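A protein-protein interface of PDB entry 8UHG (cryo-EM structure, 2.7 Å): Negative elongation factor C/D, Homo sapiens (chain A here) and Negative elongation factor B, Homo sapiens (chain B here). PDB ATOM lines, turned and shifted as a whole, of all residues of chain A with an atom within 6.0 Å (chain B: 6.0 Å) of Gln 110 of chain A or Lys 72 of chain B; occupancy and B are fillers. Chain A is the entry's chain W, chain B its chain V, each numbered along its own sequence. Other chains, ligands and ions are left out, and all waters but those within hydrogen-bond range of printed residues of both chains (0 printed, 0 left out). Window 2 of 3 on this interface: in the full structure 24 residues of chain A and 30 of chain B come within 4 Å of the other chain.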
ATOM      1  N   LEU A 101     -25.554 -13.920 -12.741  1.00  0.00           N
ATOM      2  CA  LEU A 101     -26.761 -14.355 -12.043  1.00  0.00           C
ATOM      3  C   LEU A 101     -27.929 -13.423 -12.342  1.00  0.00           C
ATOM      4  O   LEU A 101     -29.076 -13.871 -12.457  1.00  0.00           O
ATOM      5  CB  LEU A 101     -26.529 -14.447 -10.532  1.00  0.00           C
ATOM      6  CG  LEU A 101     -25.830 -15.663  -9.906  1.00  0.00           C
ATOM      7  CD1 LEU A 101     -26.141 -15.679  -8.426  1.00  0.00           C
ATOM      8  CD2 LEU A 101     -26.226 -17.012 -10.497  1.00  0.00           C
ATOM      9  N   VAL A 106     -32.889 -14.821 -12.395  1.00  0.00           N
ATOM     10  CA  VAL A 106     -33.112 -15.059 -10.973  1.00  0.00           C
ATOM     11  C   VAL A 106     -33.166 -13.713 -10.258  1.00  0.00           C
ATOM     12  O   VAL A 106     -32.506 -12.748 -10.659  1.00  0.00           O
ATOM     13  CB  VAL A 106     -32.012 -15.979 -10.397  1.00  0.00           C
ATOM     14  CG1 VAL A 106     -32.143 -16.119  -8.879  1.00  0.00           C
ATOM     15  CG2 VAL A 106     -32.067 -17.361 -11.055  1.00  0.00           C
ATOM     16  N   GLU A 107     -33.978 -13.640  -9.206  1.00  0.00           N
ATOM     17  CA  GLU A 107     -34.216 -12.376  -8.518  1.00  0.00           C
ATOM     18  C   GLU A 107     -32.920 -11.866  -7.881  1.00  0.00           C
ATOM     19  O   GLU A 107     -32.278 -12.614  -7.132  1.00  0.00           O
ATOM     20  CB  GLU A 107     -35.283 -12.560  -7.439  1.00  0.00           C
ATOM     21  CG  GLU A 107     -35.963 -11.266  -7.011  1.00  0.00           C
ATOM     22  CD  GLU A 107     -36.795 -11.419  -5.749  1.00  0.00           C
ATOM     23  OE1 GLU A 107     -36.824 -12.528  -5.174  1.00  0.00           O
ATOM     24  OE2 GLU A 107     -37.424 -10.425  -5.329  1.00  0.00           O
ATOM     25  N   PRO A 108     -32.491 -10.618  -8.145  1.00  0.00           N
ATOM     26  CA  PRO A 108     -31.303 -10.109  -7.435  1.00  0.00           C
ATOM     27  C   PRO A 108     -31.506  -9.940  -5.940  1.00  0.00           C
ATOM     28  O   PRO A 108     -30.515  -9.882  -5.200  1.00  0.00           O
ATOM     29  CB  PRO A 108     -31.034  -8.758  -8.112  1.00  0.00           C
ATOM     30  CG  PRO A 108     -32.331  -8.349  -8.669  1.00  0.00           C
ATOM     31  CD  PRO A 108     -32.997  -9.614  -9.103  1.00  0.00           C
ATOM     32  N   VAL A 109     -32.752  -9.854  -5.466  1.00  0.00           N
ATOM     33  CA  VAL A 109     -32.978  -9.723  -4.033  1.00  0.00           C
ATOM     34  C   VAL A 109     -32.594 -11.010  -3.314  1.00  0.00           C
ATOM     35  O   VAL A 109     -32.258 -10.972  -2.126  1.00  0.00           O
ATOM     36  CB  VAL A 109     -34.437  -9.329  -3.723  1.00  0.00           C
ATOM     37  CG1 VAL A 109     -34.585  -8.928  -2.249  1.00  0.00           C
ATOM     38  CG2 VAL A 109     -34.900  -8.183  -4.631  1.00  0.00           C
ATOM     39  N   GLN A 110     -32.619 -12.153  -4.008  1.00  0.00           N
ATOM     40  CA  GLN A 110     -32.031 -13.369  -3.455  1.00  0.00           C
ATOM     41  C   GLN A 110     -30.547 -13.168  -3.174  1.00  0.00           C
ATOM     42  O   GLN A 110     -30.047 -13.566  -2.114  1.00  0.00           O
ATOM     43  CB  GLN A 110     -32.247 -14.535  -4.423  1.00  0.00           C
ATOM     44  CG  GLN A 110     -31.662 -15.876  -3.978  1.00  0.00           C
ATOM     45  CD  GLN A 110     -32.006 -17.004  -4.930  1.00  0.00           C
ATOM     46  OE1 GLN A 110     -32.817 -16.839  -5.842  1.00  0.00           O
ATOM     47  NE2 GLN A 110     -31.385 -18.160  -4.726  1.00  0.00           N
ATOM     48  N   VAL A 111     -29.831 -12.536  -4.108  1.00  0.00           N
ATOM     49  CA  VAL A 111     -28.414 -12.255  -3.900  1.00  0.00           C
ATOM     50  C   VAL A 111     -28.234 -11.280  -2.744  1.00  0.00           C
ATOM     51  O   VAL A 111     -27.307 -11.418  -1.938  1.00  0.00           O
ATOM     52  CB  VAL A 111     -27.771 -11.717  -5.195  1.00  0.00           C
ATOM     53  CG1 VAL A 111     -26.303 -11.379  -4.955  1.00  0.00           C
ATOM     54  CG2 VAL A 111     -27.924 -12.722  -6.341  1.00  0.00           C
ATOM     55  N   GLN A 112     -29.109 -10.274  -2.651  1.00  0.00           N
ATOM     56  CA  GLN A 112     -29.026  -9.322  -1.544  1.00  0.00           C
ATOM     57  C   GLN A 112     -29.208 -10.023  -0.203  1.00  0.00           C
ATOM     58  O   GLN A 112     -28.443  -9.789   0.740  1.00  0.00           O
ATOM     59  CB  GLN A 112     -30.073  -8.220  -1.708  1.00  0.00           C
ATOM     60  CG  GLN A 112     -29.759  -7.188  -2.783  1.00  0.00           C
ATOM     61  CD  GLN A 112     -29.943  -5.764  -2.287  1.00  0.00           C
ATOM     62  OE1 GLN A 112     -29.377  -5.375  -1.265  1.00  0.00           O
ATOM     63  NE2 GLN A 112     -30.739  -4.982  -3.006  1.00  0.00           N
ATOM     64  N   GLU A 113     -30.215 -10.895  -0.105  1.00  0.00           N
ATOM     65  CA  GLU A 113     -30.442 -11.630   1.134  1.00  0.00           C
ATOM     66  C   GLU A 113     -29.264 -12.537   1.459  1.00  0.00           C
ATOM     67  O   GLU A 113     -28.857 -12.638   2.620  1.00  0.00           O
ATOM     68  CB  GLU A 113     -31.728 -12.451   1.044  1.00  0.00           C
ATOM     69  CG  GLU A 113     -33.008 -11.628   1.073  1.00  0.00           C
ATOM     70  CD  GLU A 113     -34.194 -12.402   1.619  1.00  0.00           C
ATOM     71  OE1 GLU A 113     -34.087 -12.956   2.734  1.00  0.00           O
ATOM     72  OE2 GLU A 113     -35.233 -12.461   0.929  1.00  0.00           O
ATOM     73  N   THR A 114     -28.701 -13.202   0.447  1.00  0.00           N
ATOM     74  CA  THR A 114     -27.576 -14.101   0.685  1.00  0.00           C
ATOM     75  C   THR A 114     -26.362 -13.339   1.204  1.00  0.00           C
ATOM     76  O   THR A 114     -25.733 -13.745   2.191  1.00  0.00           O
ATOM     77  CB  THR A 114     -27.227 -14.851  -0.601  1.00  0.00           C
ATOM     78  OG1 THR A 114     -28.368 -15.592  -1.054  1.00  0.00           O
ATOM     79  CG2 THR A 114     -26.071 -15.805  -0.365  1.00  0.00           C
ATOM     80  N   VAL A 115     -26.025 -12.219   0.557  1.00  0.00           N
ATOM     81  CA  VAL A 115     -24.865 -11.437   0.977  1.00  0.00           C
ATOM     82  C   VAL A 115     -25.088 -10.853   2.366  1.00  0.00           C
ATOM     83  O   VAL A 115     -24.178 -10.860   3.209  1.00  0.00           O
ATOM     84  CB  VAL A 115     -24.555 -10.338  -0.059  1.00  0.00           C
ATOM     85  CG1 VAL A 115     -23.460  -9.398   0.462  1.00  0.00           C
ATOM     86  CG2 VAL A 115     -24.130 -10.963  -1.381  1.00  0.00           C
ATOM     87  N   ASP B  67     -17.658 -17.599  -4.597  1.00  0.00           N
ATOM     88  CA  ASP B  67     -17.973 -19.022  -4.503  1.00  0.00           C
ATOM     89  C   ASP B  67     -19.481 -19.247  -4.568  1.00  0.00           C
ATOM     90  O   ASP B  67     -19.965 -20.073  -5.360  1.00  0.00           O
ATOM     91  CB  ASP B  67     -17.392 -19.603  -3.212  1.00  0.00           C
ATOM     92  CG  ASP B  67     -17.096 -21.088  -3.319  1.00  0.00           C
ATOM     93  OD1 ASP B  67     -17.793 -21.786  -4.085  1.00  0.00           O
ATOM     94  OD2 ASP B  67     -16.159 -21.555  -2.635  1.00  0.00           O
ATOM     95  N   GLU B  68     -20.240 -18.458  -3.794  1.00  0.00           N
ATOM     96  CA  GLU B  68     -21.698 -18.595  -3.772  1.00  0.00           C
ATOM     97  C   GLU B  68     -22.307 -18.385  -5.160  1.00  0.00           C
ATOM     98  O   GLU B  68     -23.109 -19.204  -5.642  1.00  0.00           O
ATOM     99  CB  GLU B  68     -22.282 -17.588  -2.776  1.00  0.00           C
ATOM    100  CG  GLU B  68     -23.770 -17.750  -2.466  1.00  0.00           C
ATOM    101  CD  GLU B  68     -24.070 -18.974  -1.623  1.00  0.00           C
ATOM    102  OE1 GLU B  68     -23.305 -19.246  -0.674  1.00  0.00           O
ATOM    103  OE2 GLU B  68     -25.071 -19.664  -1.909  1.00  0.00           O
ATOM    104  N   LEU B  69     -21.917 -17.304  -5.830  1.00  0.00           N
ATOM    105  CA  LEU B  69     -22.607 -16.897  -7.043  1.00  0.00           C
ATOM    106  C   LEU B  69     -22.217 -17.752  -8.247  1.00  0.00           C
ATOM    107  O   LEU B  69     -23.075 -18.005  -9.098  1.00  0.00           O
ATOM    108  CB  LEU B  69     -22.356 -15.407  -7.304  1.00  0.00           C
ATOM    109  CG  LEU B  69     -22.808 -14.420  -6.202  1.00  0.00           C
ATOM    110  CD1 LEU B  69     -22.035 -13.111  -6.335  1.00  0.00           C
ATOM    111  CD2 LEU B  69     -24.288 -14.117  -6.192  1.00  0.00           C
ATOM    112  N   ARG B  70     -20.971 -18.255  -8.337  1.00  0.00           N
ATOM    113  CA  ARG B  70     -20.716 -19.211  -9.419  1.00  0.00           C
ATOM    114  C   ARG B  70     -21.323 -20.576  -9.128  1.00  0.00           C
ATOM    115  O   ARG B  70     -21.664 -21.296 -10.077  1.00  0.00           O
ATOM    116  CB  ARG B  70     -19.226 -19.395  -9.714  1.00  0.00           C
ATOM    117  CG  ARG B  70     -18.981 -20.311 -10.932  1.00  0.00           C
ATOM    118  CD  ARG B  70     -17.564 -20.215 -11.449  1.00  0.00           C
ATOM    119  NE  ARG B  70     -16.601 -20.385 -10.368  1.00  0.00           N
ATOM    120  CZ  ARG B  70     -16.355 -21.528  -9.738  1.00  0.00           C
ATOM    121  NH1 ARG B  70     -16.958 -22.659 -10.074  1.00  0.00           N
ATOM    122  NH2 ARG B  70     -15.482 -21.536  -8.736  1.00  0.00           N
ATOM    123  N   ASP B  71     -21.464 -20.965  -7.851  1.00  0.00           N
ATOM    124  CA  ASP B  71     -22.234 -22.173  -7.563  1.00  0.00           C
ATOM    125  C   ASP B  71     -23.652 -22.039  -8.103  1.00  0.00           C
ATOM    126  O   ASP B  71     -24.164 -22.945  -8.777  1.00  0.00           O
ATOM    127  CB  ASP B  71     -22.254 -22.446  -6.057  1.00  0.00           C
ATOM    128  CG  ASP B  71     -20.908 -22.900  -5.526  1.00  0.00           C
ATOM    129  OD1 ASP B  71     -19.948 -22.989  -6.320  1.00  0.00           O
ATOM    130  OD2 ASP B  71     -20.810 -23.165  -4.310  1.00  0.00           O
ATOM    131  N   LYS B  72     -24.274 -20.881  -7.878  1.00  0.00           N
ATOM    132  CA  LYS B  72     -25.616 -20.673  -8.415  1.00  0.00           C
ATOM    133  C   LYS B  72     -25.619 -20.551  -9.938  1.00  0.00           C
ATOM    134  O   LYS B  72     -26.590 -20.965 -10.582  1.00  0.00           O
ATOM    135  CB  LYS B  72     -26.252 -19.448  -7.766  1.00  0.00           C
ATOM    136  CG  LYS B  72     -26.788 -19.764  -6.386  1.00  0.00           C
ATOM    137  CD  LYS B  72     -27.264 -18.540  -5.633  1.00  0.00           C
ATOM    138  CE  LYS B  72     -27.602 -18.901  -4.192  1.00  0.00           C
ATOM    139  NZ  LYS B  72     -28.646 -19.963  -4.095  1.00  0.00           N
ATOM    140  N   LEU B  73     -24.561 -19.998 -10.538  1.00  0.00           N
ATOM    141  CA  LEU B  73     -24.514 -19.913 -11.998  1.00  0.00           C
ATOM    142  C   LEU B  73     -24.430 -21.299 -12.630  1.00  0.00           C
ATOM    143  O   LEU B  73     -25.078 -21.559 -13.650  1.00  0.00           O
ATOM    144  CB  LEU B  73     -23.334 -19.046 -12.451  1.00  0.00           C
ATOM    145  CG  LEU B  73     -23.131 -18.864 -13.966  1.00  0.00           C
ATOM    146  CD1 LEU B  73     -24.379 -18.307 -14.649  1.00  0.00           C
ATOM    147  CD2 LEU B  73     -21.935 -17.965 -14.251  1.00  0.00           C
ATOM    148  N   LEU B  74     -23.627 -22.196 -12.054  1.00  0.00           N
ATOM    149  CA  LEU B  74     -23.583 -23.569 -12.557  1.00  0.00           C
ATOM    150  C   LEU B  74     -24.919 -24.275 -12.345  1.00  0.00           C
ATOM    151  O   LEU B  74     -25.388 -25.020 -13.226  1.00  0.00           O
ATOM    152  CB  LEU B  74     -22.450 -24.339 -11.877  1.00  0.00           C
ATOM    153  CG  LEU B  74     -21.078 -24.128 -12.525  1.00  0.00           C
ATOM    154  CD1 LEU B  74     -19.955 -24.150 -11.496  1.00  0.00           C
ATOM    155  CD2 LEU B  74     -20.819 -25.169 -13.612  1.00  0.00           C
ATOM    156  N   GLU B  75     -25.543 -24.049 -11.181  1.00  0.00           N
ATOM    157  CA  GLU B  75     -26.878 -24.585 -10.925  1.00  0.00           C
ATOM    158  C   GLU B  75     -27.862 -24.143 -11.997  1.00  0.00           C
ATOM    159  O   GLU B  75     -28.653 -24.947 -12.501  1.00  0.00           O
ATOM    160  CB  GLU B  75     -27.370 -24.128  -9.550  1.00  0.00           C
ATOM    161  CG  GLU B  75     -26.678 -24.798  -8.378  1.00  0.00           C
ATOM    162  CD  GLU B  75     -26.844 -24.019  -7.088  1.00  0.00           C
ATOM    163  OE1 GLU B  75     -27.974 -23.568  -6.806  1.00  0.00           O
ATOM    164  OE2 GLU B  75     -25.842 -23.849  -6.360  1.00  0.00           O
ATOM    165  N   ARG B  76     -27.804 -22.870 -12.384  1.00  0.00           N
ATOM    166  CA  ARG B  76     -28.733 -22.355 -13.380  1.00  0.00           C
ATOM    167  C   ARG B  76     -28.350 -22.760 -14.799  1.00  0.00           C
ATOM    168  O   ARG B  76     -29.218 -22.798 -15.668  1.00  0.00           O
ATOM    169  CB  ARG B  76     -28.822 -20.838 -13.272  1.00  0.00           C
ATOM    170  CG  ARG B  76     -29.840 -20.180 -14.187  1.00  0.00           C
ATOM    171  CD  ARG B  76     -31.287 -20.635 -13.980  1.00  0.00           C
ATOM    172  NE  ARG B  76     -32.224 -19.634 -14.485  1.00  0.00           N
ATOM    173  CZ  ARG B  76     -33.487 -19.851 -14.841  1.00  0.00           C
ATOM    174  NH1 ARG B  76     -34.037 -21.056 -14.788  1.00  0.00           N
ATOM    175  NH2 ARG B  76     -34.219 -18.828 -15.272  1.00  0.00           N
ATOM    176  N   VAL B  77     -27.076 -23.052 -15.065  1.00  0.00           N
ATOM    177  CA  VAL B  77     -26.721 -23.656 -16.349  1.00  0.00           C
ATOM    178  C   VAL B  77     -27.416 -25.004 -16.485  1.00  0.00           C
ATOM    179  O   VAL B  77     -28.069 -25.291 -17.499  1.00  0.00           O
ATOM    180  CB  VAL B  77     -25.188 -23.778 -16.483  1.00  0.00           C
ATOM    181  CG1 VAL B  77     -24.776 -24.845 -17.520  1.00  0.00           C
ATOM    182  CG2 VAL B  77     -24.592 -22.432 -16.866  1.00  0.00           C
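Among the printed residues, pairs that only touch across the chains: Leu 101 of chain A with Leu 69 of chain B (3.3 Å), Leu 101 of chain A with Lys 72 of chain B (3.6 Å), Leu 101 of chain A with Leu 73 of chain B (3.4 Å), Val 111 of chain A with Leu 69 of chain B (3.6 Å) and Thr 114 of chain A with Glu 68 of chain B (3.7 Å).
The side-chain hydroxyl (OG1) of Thr 114 of chain A sits at hydrogen-bond distance from the backbone carbonyl oxygen (O) of Gln 110 of chain A (2.8 Å).
Gln 110 of chain A touches just one residue of chain B: Lys 72 (3.3 Å). Of chain A, only Leu 101 and Gln 110 come within 4 Å of Lys 72 of chain B. Printed residues of chain B within 4 Å of Thr 114 of chain A: Glu 68 (3.7 Å). Of the printed residues of chain A, Leu 73 of chain B touches Leu 101 (3.4 Å). Printed residues of chain A within 4 Å of Leu 69 of chain B: Leu 101 and Val 111. The nearest printed residue of chain B that does not touch Gln 110 of chain A is Glu 75 of chain B (6.7 Å). The nearest residue of chain A that does not touch Lys 72 of chain B is Thr 114 of chain A (4.6 Å). The nearest printed residue of chain A that does not touch Leu 73 of chain B is Val 106 of chain A (8.0 Å).
The side-chain amino group (NZ) of Lys 72 of chain B sits close to the side-chain amide nitrogen (NE2) of Gln 110 of chain A, 3.3 Å away.
Of the 11 printed residues of chain A, 4 touch a printed residue of chain B. Of the 11 printed residues of chain B, 4 touch a printed residue of chain A. Among the printed residues, no Asp or Glu carboxylate lies within 4 Å of a Lys or Arg side-chain nitrogen of the other chain.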
